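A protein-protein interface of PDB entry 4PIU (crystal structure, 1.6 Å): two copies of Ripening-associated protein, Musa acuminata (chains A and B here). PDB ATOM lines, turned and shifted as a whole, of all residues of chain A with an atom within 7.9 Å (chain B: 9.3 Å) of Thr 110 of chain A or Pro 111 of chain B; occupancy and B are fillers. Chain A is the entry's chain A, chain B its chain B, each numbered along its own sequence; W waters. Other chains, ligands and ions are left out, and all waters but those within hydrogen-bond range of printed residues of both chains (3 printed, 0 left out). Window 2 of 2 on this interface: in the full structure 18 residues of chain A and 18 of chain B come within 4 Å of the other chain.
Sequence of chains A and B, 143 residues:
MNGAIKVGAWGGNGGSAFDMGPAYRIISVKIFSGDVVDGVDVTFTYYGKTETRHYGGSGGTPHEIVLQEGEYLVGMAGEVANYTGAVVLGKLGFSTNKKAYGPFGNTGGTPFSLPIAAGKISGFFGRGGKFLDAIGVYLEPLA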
ATOM      1  N   TRP A  10     -22.055 -19.536   6.172  1.00  0.00           N
ATOM      2  CA  TRP A  10     -20.745 -19.947   6.685  1.00  0.00           C
ATOM      3  C   TRP A  10     -20.155 -20.971   5.720  1.00  0.00           C
ATOM      4  O   TRP A  10     -20.862 -21.896   5.296  1.00  0.00           O
ATOM      5  CB  TRP A  10     -20.943 -20.602   8.063  1.00  0.00           C
ATOM      6  CG  TRP A  10     -21.360 -19.613   9.087  1.00  0.00           C
ATOM      7  CD1 TRP A  10     -20.538 -18.839   9.862  1.00  0.00           C
ATOM      8  CD2 TRP A  10     -22.703 -19.302   9.484  1.00  0.00           C
ATOM      9  NE1 TRP A  10     -21.287 -18.038  10.695  1.00  0.00           N
ATOM     10  CE2 TRP A  10     -22.621 -18.312  10.483  1.00  0.00           C
ATOM     11  CE3 TRP A  10     -23.976 -19.761   9.076  1.00  0.00           C
ATOM     12  CZ2 TRP A  10     -23.757 -17.775  11.103  1.00  0.00           C
ATOM     13  CZ3 TRP A  10     -25.099 -19.231   9.687  1.00  0.00           C
ATOM     14  CH2 TRP A  10     -24.987 -18.239  10.697  1.00  0.00           C
ATOM     15  N   GLY A  11     -18.874 -20.823   5.380  1.00  0.00           N
ATOM     16  CA  GLY A  11     -18.246 -21.763   4.460  1.00  0.00           C
ATOM     17  C   GLY A  11     -17.370 -21.042   3.458  1.00  0.00           C
ATOM     18  O   GLY A  11     -16.983 -19.882   3.672  1.00  0.00           O
ATOM     19  N   GLY A  78     -21.466 -25.675  13.318  1.00  0.00           N
ATOM     20  CA  GLY A  78     -20.596 -26.555  12.517  1.00  0.00           C
ATOM     21  C   GLY A  78     -19.180 -26.028  12.473  1.00  0.00           C
ATOM     22  O   GLY A  78     -18.779 -25.226  13.321  1.00  0.00           O
ATOM     23  N   GLU A  79     -18.399 -26.563  11.548  1.00  0.00           N
ATOM     24  CA  GLU A  79     -17.019 -26.113  11.393  1.00  0.00           C
ATOM     25  C   GLU A  79     -16.764 -25.998   9.919  1.00  0.00           C
ATOM     26  O   GLU A  79     -17.194 -26.870   9.116  1.00  0.00           O
ATOM     27  CB  GLU A  79     -16.056 -27.141  12.003  1.00  0.00           C
ATOM     28  CG  GLU A  79     -16.337 -27.324  13.497  1.00  0.00           C
ATOM     29  CD  GLU A  79     -15.211 -27.936  14.323  1.00  0.00           C
ATOM     30  OE1 GLU A  79     -14.144 -28.302  13.816  1.00  0.00           O
ATOM     31  OE2 GLU A  79     -15.435 -28.089  15.534  1.00  0.00           O
ATOM     32  N   VAL A  80     -16.039 -24.949   9.557  1.00  0.00           N
ATOM     33  CA  VAL A  80     -15.625 -24.737   8.169  1.00  0.00           C
ATOM     34  C   VAL A  80     -14.192 -25.240   7.993  1.00  0.00           C
ATOM     35  O   VAL A  80     -13.278 -24.801   8.712  1.00  0.00           O
ATOM     36  CB  VAL A  80     -15.735 -23.234   7.793  1.00  0.00           C
ATOM     37  CG1 VAL A  80     -15.200 -22.994   6.382  1.00  0.00           C
ATOM     38  CG2 VAL A  80     -17.179 -22.746   7.926  1.00  0.00           C
ATOM     39  N   ALA A  81     -14.007 -26.146   7.031  1.00  0.00           N
ATOM     40  CA  ALA A  81     -12.777 -26.929   6.937  1.00  0.00           C
ATOM     41  C   ALA A  81     -12.224 -26.872   5.547  1.00  0.00           C
ATOM     42  O   ALA A  81     -12.959 -26.615   4.611  1.00  0.00           O
ATOM     43  CB  ALA A  81     -13.064 -28.393   7.272  1.00  0.00           C
ATOM     44  N   ASN A  82     -10.933 -27.147   5.422  1.00  0.00           N
ATOM     45  CA  ASN A  82     -10.366 -27.385   4.104  1.00  0.00           C
ATOM     46  C   ASN A  82     -10.318 -28.892   3.886  1.00  0.00           C
ATOM     47  O   ASN A  82      -9.667 -29.616   4.674  1.00  0.00           O
ATOM     48  CB  ASN A  82      -8.958 -26.799   4.004  1.00  0.00           C
ATOM     49  CG  ASN A  82      -8.432 -26.834   2.584  1.00  0.00           C
ATOM     50  OD1 ASN A  82      -8.201 -27.904   2.005  1.00  0.00           O
ATOM     51  ND2 ASN A  82      -8.197 -25.652   2.029  1.00  0.00           N
ATOM     52  N   VAL A  88     -15.156 -25.955   2.857  1.00  0.00           N
ATOM     53  CA  VAL A  88     -16.520 -26.561   2.931  1.00  0.00           C
ATOM     54  C   VAL A  88     -16.962 -26.725   4.355  1.00  0.00           C
ATOM     55  O   VAL A  88     -16.210 -26.438   5.299  1.00  0.00           O
ATOM     56  CB  VAL A  88     -16.553 -27.966   2.223  1.00  0.00           C
ATOM     57  CG1 VAL A  88     -16.142 -27.835   0.757  1.00  0.00           C
ATOM     58  CG2 VAL A  88     -15.622 -28.950   2.919  1.00  0.00           C
ATOM     59  N   LEU A  89     -18.190 -27.183   4.540  1.00  0.00           N
ATOM     60  CA  LEU A  89     -18.630 -27.590   5.882  1.00  0.00           C
ATOM     61  C   LEU A  89     -17.985 -28.941   6.222  1.00  0.00           C
ATOM     62  O   LEU A  89     -18.313 -29.963   5.624  1.00  0.00           O
ATOM     63  CB  LEU A  89     -20.149 -27.687   5.946  1.00  0.00           C
ATOM     64  CG  LEU A  89     -20.952 -26.389   6.158  1.00  0.00           C
ATOM     65  CD1 LEU A  89     -20.673 -25.779   7.534  1.00  0.00           C
ATOM     66  CD2 LEU A  89     -20.712 -25.368   5.081  1.00  0.00           C
ATOM     67  N   GLY A  90     -17.075 -28.919   7.189  1.00  0.00           N
ATOM     68  CA  GLY A  90     -16.420 -30.136   7.650  1.00  0.00           C
ATOM     69  C   GLY A  90     -17.314 -30.890   8.625  1.00  0.00           C
ATOM     70  O   GLY A  90     -17.200 -32.106   8.719  1.00  0.00           O
ATOM     71  N   LYS A  91     -18.148 -30.144   9.357  1.00  0.00           N
ATOM     72  CA  LYS A  91     -19.079 -30.668  10.384  1.00  0.00           C
ATOM     73  C   LYS A  91     -20.293 -29.760  10.351  1.00  0.00           C
ATOM     74  O   LYS A  91     -20.148 -28.553  10.123  1.00  0.00           O
ATOM     75  CB  LYS A  91     -18.467 -30.610  11.810  1.00  0.00           C
ATOM     76  CG  LYS A  91     -17.244 -31.474  11.985  1.00  0.00           C
ATOM     77  CD  LYS A  91     -16.851 -31.520  13.421  1.00  0.00           C
ATOM     78  CE  LYS A  91     -15.527 -32.245  13.487  1.00  0.00           C
ATOM     79  NZ  LYS A  91     -15.259 -32.670  14.887  1.00  0.00           N
ATOM     80  N   THR A 107     -14.474 -33.474   9.849  1.00  0.00           N
ATOM     81  CA  THR A 107     -13.267 -32.675   9.575  1.00  0.00           C
ATOM     82  C   THR A 107     -13.311 -31.353  10.307  1.00  0.00           C
ATOM     83  O   THR A 107     -14.195 -30.526  10.081  1.00  0.00           O
ATOM     84  CB  THR A 107     -13.046 -32.474   8.059  1.00  0.00           C
ATOM     85  OG1 THR A 107     -13.004 -33.763   7.434  1.00  0.00           O
ATOM     86  CG2 THR A 107     -11.711 -31.761   7.786  1.00  0.00           C
ATOM     87  N   GLY A 108     -12.355 -31.182  11.214  1.00  0.00           N
ATOM     88  CA  GLY A 108     -12.298 -29.965  12.003  1.00  0.00           C
ATOM     89  C   GLY A 108     -11.835 -28.746  11.225  1.00  0.00           C
ATOM     90  O   GLY A 108     -11.101 -28.838  10.223  1.00  0.00           O
ATOM     91  N   GLY A 109     -12.232 -27.579  11.718  1.00  0.00           N
ATOM     92  CA  GLY A 109     -11.812 -26.354  11.105  1.00  0.00           C
ATOM     93  C   GLY A 109     -12.290 -25.272  12.020  1.00  0.00           C
ATOM     94  O   GLY A 109     -12.256 -25.453  13.255  1.00  0.00           O
ATOM     95  N   THR A 110     -12.792 -24.197  11.430  1.00  0.00           N
ATOM     96  CA  THR A 110     -13.174 -22.981  12.163  1.00  0.00           C
ATOM     97  C   THR A 110     -14.620 -23.099  12.593  1.00  0.00           C
ATOM     98  O   THR A 110     -15.518 -23.123  11.750  1.00  0.00           O
ATOM     99  CB  THR A 110     -13.053 -21.740  11.272  1.00  0.00           C
ATOM    100  OG1 THR A 110     -11.713 -21.627  10.760  1.00  0.00           O
ATOM    101  CG2 THR A 110     -13.405 -20.464  12.050  1.00  0.00           C
ATOM    102  N   PRO A 111     -14.868 -23.147  13.906  1.00  0.00           N
ATOM    103  CA  PRO A 111     -16.242 -23.278  14.344  1.00  0.00           C
ATOM    104  C   PRO A 111     -17.115 -22.068  14.082  1.00  0.00           C
ATOM    105  O   PRO A 111     -16.641 -20.916  14.075  1.00  0.00           O
ATOM    106  CB  PRO A 111     -16.121 -23.441  15.856  1.00  0.00           C
ATOM    107  CG  PRO A 111     -14.703 -23.564  16.191  1.00  0.00           C
ATOM    108  CD  PRO A 111     -13.891 -23.168  15.002  1.00  0.00           C
ATOM    109  N   PHE A 112     -18.401 -22.362  13.903  1.00  0.00           N
ATOM    110  CA  PHE A 112     -19.441 -21.332  13.972  1.00  0.00           C
ATOM    111  C   PHE A 112     -20.650 -21.911  14.707  1.00  0.00           C
ATOM    112  O   PHE A 112     -20.792 -23.151  14.853  1.00  0.00           O
ATOM    113  CB  PHE A 112     -19.878 -20.833  12.589  1.00  0.00           C
ATOM    114  CG  PHE A 112     -20.676 -21.842  11.812  1.00  0.00           C
ATOM    115  CD1 PHE A 112     -22.064 -21.839  11.883  1.00  0.00           C
ATOM    116  CD2 PHE A 112     -20.023 -22.813  11.054  1.00  0.00           C
ATOM    117  CE1 PHE A 112     -22.802 -22.794  11.183  1.00  0.00           C
ATOM    118  CE2 PHE A 112     -20.757 -23.785  10.380  1.00  0.00           C
ATOM    119  CZ  PHE A 112     -22.131 -23.770  10.446  1.00  0.00           C
ATOM    120  N   SER A 113     -21.511 -21.008  15.171  1.00  0.00           N
ATOM    121  CA  SER A 113     -22.671 -21.463  15.948  1.00  0.00           C
ATOM    122  C   SER A 113     -23.757 -20.419  15.832  1.00  0.00           C
ATOM    123  O   SER A 113     -23.481 -19.180  15.843  1.00  0.00           O
ATOM    124  CB  SER A 113     -22.292 -21.692  17.409  1.00  0.00           C
ATOM    125  OG  SER A 113     -21.730 -20.493  17.988  1.00  0.00           O
ATOM    126  N   TRP B  10     -23.857 -15.435  22.462  1.00  0.00           N
ATOM    127  CA  TRP B  10     -22.543 -16.115  22.460  1.00  0.00           C
ATOM    128  C   TRP B  10     -21.791 -15.683  23.690  1.00  0.00           C
ATOM    129  O   TRP B  10     -21.727 -14.490  24.019  1.00  0.00           O
ATOM    130  CB  TRP B  10     -21.786 -15.676  21.188  1.00  0.00           C
ATOM    131  CG  TRP B  10     -22.378 -16.241  19.964  1.00  0.00           C
ATOM    132  CD1 TRP B  10     -22.063 -17.437  19.372  1.00  0.00           C
ATOM    133  CD2 TRP B  10     -23.350 -15.616  19.119  1.00  0.00           C
ATOM    134  NE1 TRP B  10     -22.814 -17.624  18.226  1.00  0.00           N
ATOM    135  CE2 TRP B  10     -23.602 -16.508  18.037  1.00  0.00           C
ATOM    136  CE3 TRP B  10     -24.015 -14.381  19.151  1.00  0.00           C
ATOM    137  CZ2 TRP B  10     -24.502 -16.210  17.019  1.00  0.00           C
ATOM    138  CZ3 TRP B  10     -24.931 -14.095  18.134  1.00  0.00           C
ATOM    139  CH2 TRP B  10     -25.183 -15.006  17.091  1.00  0.00           C
ATOM    140  N   GLY B  11     -21.199 -16.661  24.375  1.00  0.00           N
ATOM    141  CA  GLY B  11     -20.445 -16.363  25.579  1.00  0.00           C
ATOM    142  C   GLY B  11     -20.739 -17.363  26.655  1.00  0.00           C
ATOM    143  O   GLY B  11     -21.143 -18.499  26.382  1.00  0.00           O
ATOM    144  N   MET B  76     -21.703  -9.249  13.261  1.00  0.00           N
ATOM    145  CA  MET B  76     -21.042  -9.278  14.569  1.00  0.00           C
ATOM    146  C   MET B  76     -20.157 -10.512  14.624  1.00  0.00           C
ATOM    147  O   MET B  76     -20.500 -11.542  14.039  1.00  0.00           O
ATOM    148  CB  MET B  76     -22.092  -9.314  15.690  1.00  0.00           C
ATOM    149  CG  MET B  76     -21.507  -9.241  17.111  1.00  0.00           C
ATOM    150  SD  MET B  76     -22.790  -9.123  18.389  1.00  0.00           S
ATOM    151  CE  MET B  76     -23.488 -10.773  18.302  1.00  0.00           C
ATOM    152  N   ALA B  77     -19.001 -10.425  15.283  1.00  0.00           N
ATOM    153  CA  ALA B  77     -18.108 -11.572  15.353  1.00  0.00           C
ATOM    154  C   ALA B  77     -17.213 -11.407  16.551  1.00  0.00           C
ATOM    155  O   ALA B  77     -17.141 -10.339  17.143  1.00  0.00           O
ATOM    156  CB  ALA B  77     -17.273 -11.736  14.071  1.00  0.00           C
ATOM    157  N   GLY B  78     -16.582 -12.494  16.944  1.00  0.00           N
ATOM    158  CA  GLY B  78     -15.679 -12.416  18.092  1.00  0.00           C
ATOM    159  C   GLY B  78     -15.198 -13.774  18.525  1.00  0.00           C
ATOM    160  O   GLY B  78     -15.214 -14.722  17.737  1.00  0.00           O
ATOM    161  N   GLU B  79     -14.713 -13.847  19.767  1.00  0.00           N
ATOM    162  CA  GLU B  79     -14.181 -15.083  20.344  1.00  0.00           C
ATOM    163  C   GLU B  79     -14.713 -15.221  21.741  1.00  0.00           C
ATOM    164  O   GLU B  79     -14.794 -14.232  22.497  1.00  0.00           O
ATOM    165  CB  GLU B  79     -12.646 -15.047  20.484  1.00  0.00           C
ATOM    166  CG  GLU B  79     -11.966 -14.827  19.149  1.00  0.00           C
ATOM    167  CD  GLU B  79     -11.500 -16.105  18.493  1.00  0.00           C
ATOM    168  OE1 GLU B  79     -11.520 -17.187  19.145  1.00  0.00           O
ATOM    169  OE2 GLU B  79     -11.083 -16.024  17.319  1.00  0.00           O
ATOM    170  N   VAL B  80     -15.096 -16.442  22.078  1.00  0.00           N
ATOM    171  CA  VAL B  80     -15.507 -16.744  23.449  1.00  0.00           C
ATOM    172  C   VAL B  80     -14.288 -17.370  24.138  1.00  0.00           C
ATOM    173  O   VAL B  80     -13.733 -18.355  23.641  1.00  0.00           O
ATOM    174  CB  VAL B  80     -16.720 -17.687  23.473  1.00  0.00           C
ATOM    175  CG1 VAL B  80     -17.047 -18.100  24.887  1.00  0.00           C
ATOM    176  CG2 VAL B  80     -17.979 -17.037  22.847  1.00  0.00           C
ATOM    177  N   ALA B  81     -13.870 -16.799  25.267  1.00  0.00           N
ATOM    178  CA  ALA B  81     -12.615 -17.164  25.917  1.00  0.00           C
ATOM    179  C   ALA B  81     -12.832 -17.574  27.331  1.00  0.00           C
ATOM    180  O   ALA B  81     -13.776 -17.147  27.971  1.00  0.00           O
ATOM    181  CB  ALA B  81     -11.676 -15.954  25.914  1.00  0.00           C
ATOM    182  N   LEU B  89     -16.636 -12.938  26.612  1.00  0.00           N
ATOM    183  CA  LEU B  89     -16.204 -12.486  25.280  1.00  0.00           C
ATOM    184  C   LEU B  89     -14.758 -12.055  25.368  1.00  0.00           C
ATOM    185  O   LEU B  89     -14.439 -11.087  26.073  1.00  0.00           O
ATOM    186  CB  LEU B  89     -17.036 -11.294  24.799  1.00  0.00           C
ATOM    187  CG  LEU B  89     -18.327 -11.554  24.032  1.00  0.00           C
ATOM    188  CD1 LEU B  89     -18.104 -12.414  22.782  1.00  0.00           C
ATOM    189  CD2 LEU B  89     -19.245 -12.232  25.023  1.00  0.00           C
ATOM    190  N   GLY B  90     -13.876 -12.770  24.674  1.00  0.00           N
ATOM    191  CA  GLY B  90     -12.471 -12.370  24.641  1.00  0.00           C
ATOM    192  C   GLY B  90     -12.205 -11.329  23.571  1.00  0.00           C
ATOM    193  O   GLY B  90     -11.230 -10.588  23.682  1.00  0.00           O
ATOM    194  N   LYS B  91     -13.003 -11.355  22.492  1.00  0.00           N
ATOM    195  CA  LYS B  91     -12.927 -10.380  21.391  1.00  0.00           C
ATOM    196  C   LYS B  91     -14.338 -10.142  20.836  1.00  0.00           C
ATOM    197  O   LYS B  91     -15.176 -11.049  20.860  1.00  0.00           O
ATOM    198  CB  LYS B  91     -12.058 -10.891  20.235  1.00  0.00           C
ATOM    199  CG  LYS B  91     -10.619 -11.258  20.611  1.00  0.00           C
ATOM    200  CD  LYS B  91      -9.798 -11.546  19.348  1.00  0.00           C
ATOM    201  CE  LYS B  91      -8.390 -11.918  19.750  1.00  0.00           C
ATOM    202  NZ  LYS B  91      -7.551 -12.053  18.490  1.00  0.00           N
ATOM    203  N   THR B 107      -8.016 -11.784  23.668  1.00  0.00           N
ATOM    204  CA  THR B 107      -7.945 -13.203  24.059  1.00  0.00           C
ATOM    205  C   THR B 107      -8.790 -14.072  23.147  1.00  0.00           C
ATOM    206  O   THR B 107     -10.010 -13.883  23.046  1.00  0.00           O
ATOM    207  CB  THR B 107      -8.389 -13.386  25.518  1.00  0.00           C
ATOM    208  OG1 THR B 107      -7.624 -12.510  26.345  1.00  0.00           O
ATOM    209  CG2 THR B 107      -8.172 -14.832  26.004  1.00  0.00           C
ATOM    210  N   GLY B 108      -8.142 -15.033  22.498  1.00  0.00           N
ATOM    211  CA  GLY B 108      -8.853 -15.959  21.620  1.00  0.00           C
ATOM    212  C   GLY B 108      -9.462 -17.110  22.382  1.00  0.00           C
ATOM    213  O   GLY B 108      -9.195 -17.285  23.562  1.00  0.00           O
ATOM    214  N   GLY B 109     -10.240 -17.928  21.697  1.00  0.00           N
ATOM    215  CA  GLY B 109     -10.862 -19.097  22.316  1.00  0.00           C
ATOM    216  C   GLY B 109     -11.666 -19.841  21.267  1.00  0.00           C
ATOM    217  O   GLY B 109     -11.097 -20.557  20.432  1.00  0.00           O
ATOM    218  N   THR B 110     -12.980 -19.714  21.327  1.00  0.00           N
ATOM    219  CA  THR B 110     -13.819 -20.329  20.310  1.00  0.00           C
ATOM    220  C   THR B 110     -14.441 -19.211  19.484  1.00  0.00           C
ATOM    221  O   THR B 110     -15.207 -18.408  20.017  1.00  0.00           O
ATOM    222  CB  THR B 110     -14.928 -21.160  20.945  1.00  0.00           C
ATOM    223  OG1 THR B 110     -14.328 -22.183  21.756  1.00  0.00           O
ATOM    224  CG2 THR B 110     -15.839 -21.789  19.870  1.00  0.00           C
ATOM    225  N   PRO B 111     -14.122 -19.161  18.168  1.00  0.00           N
ATOM    226  CA  PRO B 111     -14.692 -18.076  17.363  1.00  0.00           C
ATOM    227  C   PRO B 111     -16.190 -18.230  17.131  1.00  0.00           C
ATOM    228  O   PRO B 111     -16.734 -19.368  17.139  1.00  0.00           O
ATOM    229  CB  PRO B 111     -13.938 -18.188  16.027  1.00  0.00           C
ATOM    230  CG  PRO B 111     -13.557 -19.605  15.931  1.00  0.00           C
ATOM    231  CD  PRO B 111     -13.256 -20.066  17.368  1.00  0.00           C
ATOM    232  N   PHE B 112     -16.854 -17.090  16.988  1.00  0.00           N
ATOM    233  CA  PHE B 112     -18.206 -17.033  16.440  1.00  0.00           C
ATOM    234  C   PHE B 112     -18.280 -15.921  15.412  1.00  0.00           C
ATOM    235  O   PHE B 112     -17.449 -14.988  15.398  1.00  0.00           O
ATOM    236  CB  PHE B 112     -19.265 -16.833  17.535  1.00  0.00           C
ATOM    237  CG  PHE B 112     -19.227 -15.471  18.178  1.00  0.00           C
ATOM    238  CD1 PHE B 112     -20.079 -14.456  17.725  1.00  0.00           C
ATOM    239  CD2 PHE B 112     -18.348 -15.206  19.224  1.00  0.00           C
ATOM    240  CE1 PHE B 112     -20.047 -13.172  18.328  1.00  0.00           C
ATOM    241  CE2 PHE B 112     -18.305 -13.952  19.827  1.00  0.00           C
ATOM    242  CZ  PHE B 112     -19.149 -12.915  19.365  1.00  0.00           C
ATOM    243  N   SER B 113     -19.280 -16.022  14.540  1.00  0.00           N
ATOM    244  CA  SER B 113     -19.464 -15.049  13.486  1.00  0.00           C
ATOM    245  C   SER B 113     -20.908 -15.016  13.044  1.00  0.00           C
ATOM    246  O   SER B 113     -21.563 -16.071  12.921  1.00  0.00           O
ATOM    247  CB  SER B 113     -18.569 -15.369  12.290  1.00  0.00           C
ATOM    248  OG  SER B 113     -18.768 -16.687  11.788  1.00  0.00           O
ATOM    249  N   LEU B 114     -21.398 -13.796  12.838  1.00  0.00           N
ATOM    250  CA  LEU B 114     -22.761 -13.612  12.397  1.00  0.00           C
ATOM    251  C   LEU B 114     -22.738 -12.689  11.192  1.00  0.00           C
ATOM    252  O   LEU B 114     -22.937 -11.476  11.315  1.00  0.00           O
ATOM    253  CB  LEU B 114     -23.628 -13.071  13.551  1.00  0.00           C
ATOM    254  CG  LEU B 114     -25.099 -12.890  13.148  1.00  0.00           C
ATOM    255  CD1 LEU B 114     -25.846 -14.248  13.123  1.00  0.00           C
ATOM    256  CD2 LEU B 114     -25.802 -11.912  14.146  1.00  0.00           C
HETATM  257  O   HOH W   1     -16.943 -18.511  12.885  1.00  0.00           O
HETATM  258  O   HOH W   2     -21.315 -18.169  14.699  1.00  0.00           O
HETATM  259  O   HOH W   3     -18.963 -20.674  17.760  1.00  0.00           O
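The indole nitrogen (NE1) of Trp 10 of chain B sits at hydrogen-bond distance from the backbone carbonyl oxygen (O) of Ser 113 of chain A (2.9 Å).
The indole nitrogen (NE1) of Trp 10 of chain A is in hydrogen-bond range of the backbone carbonyl oxygen (O) of Ser 113 of chain B.
O of Pro 111 of chain A sits close to O of Pro 111 of chain B, at 3.4 Å.
N of Thr 110 of chain A is in hydrogen-bond range of O of Val 80 of chain A (2.8 Å).
Among the printed residues, pairs that only touch across the chains: Thr 110 of chain A with Pro 111 of chain B (3.98 Å).
Thr 110 of chain A touches just one residue of chain B: Pro 111 (3.98 Å).
Of chain A, only Thr 110 and Pro 111 come within 4 Å of Pro 111 of chain B.
Pro 111 of chain A touches one residue of chain B.
Printed residues of chain A within 4 Å of Ser 113 of chain B: Trp 10.
Of the printed residues of chain B, Trp 10 of chain A touches Ser 113.
Of the printed residues of chain A, Trp 10 of chain B touches Ser 113.
Of the printed residues of chain B, Ser 113 of chain A touches Trp 10.
The nearest residue of chain B that does not touch Thr 110 of chain A is Ser 113 of chain B (6.6 Å).
The nearest printed residue of chain A that does not touch Ser 113 of chain B is Phe 112 of chain A (4.4 Å).
Hydrophobic or aromatic side chains of chain B that line the printed part of chain A: Trp 10 and Pro 111.
Printed residues of chain A that touch a printed residue of chain B: Trp 10, Thr 110, Pro 111 and Ser 113.
Among the printed residues, 4 pairs touch across the chains.
Trp 10 of chain A touches Ser 113 of chain B, and with the chains exchanged Ser 113 of chain A touches Trp 10 of chain B.
Thr 110 of chain A touches Pro 111 of chain B, but with the chains exchanged Pro 111 of chain A does not touch Thr 110 of chain B (4.2 Å).
Pro 111 of chain B touches its own counterpart, Pro 111 of chain A.
Positions printed for both chains: 10, 11, 78, 79, 80, 81, 89, 90, 91, 107, 108, 109, 110, 111, 112 and 113.
Water W2 bridges O of Ser 113 of chain A (2.6 Å) and O of Ser 113 of chain B (2.8 Å).
Water W3 lies within hydrogen-bond range of the backbone carbonyl oxygen (O) of Pro 111 of chain B (2.7 Å) and the side-chain hydroxyl (OG) of Ser 113 of chain A (2.8 Å).
Water W1 lies within hydrogen-bond range of O of Pro 111 of chain A and OG of Ser 113 of chain B.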
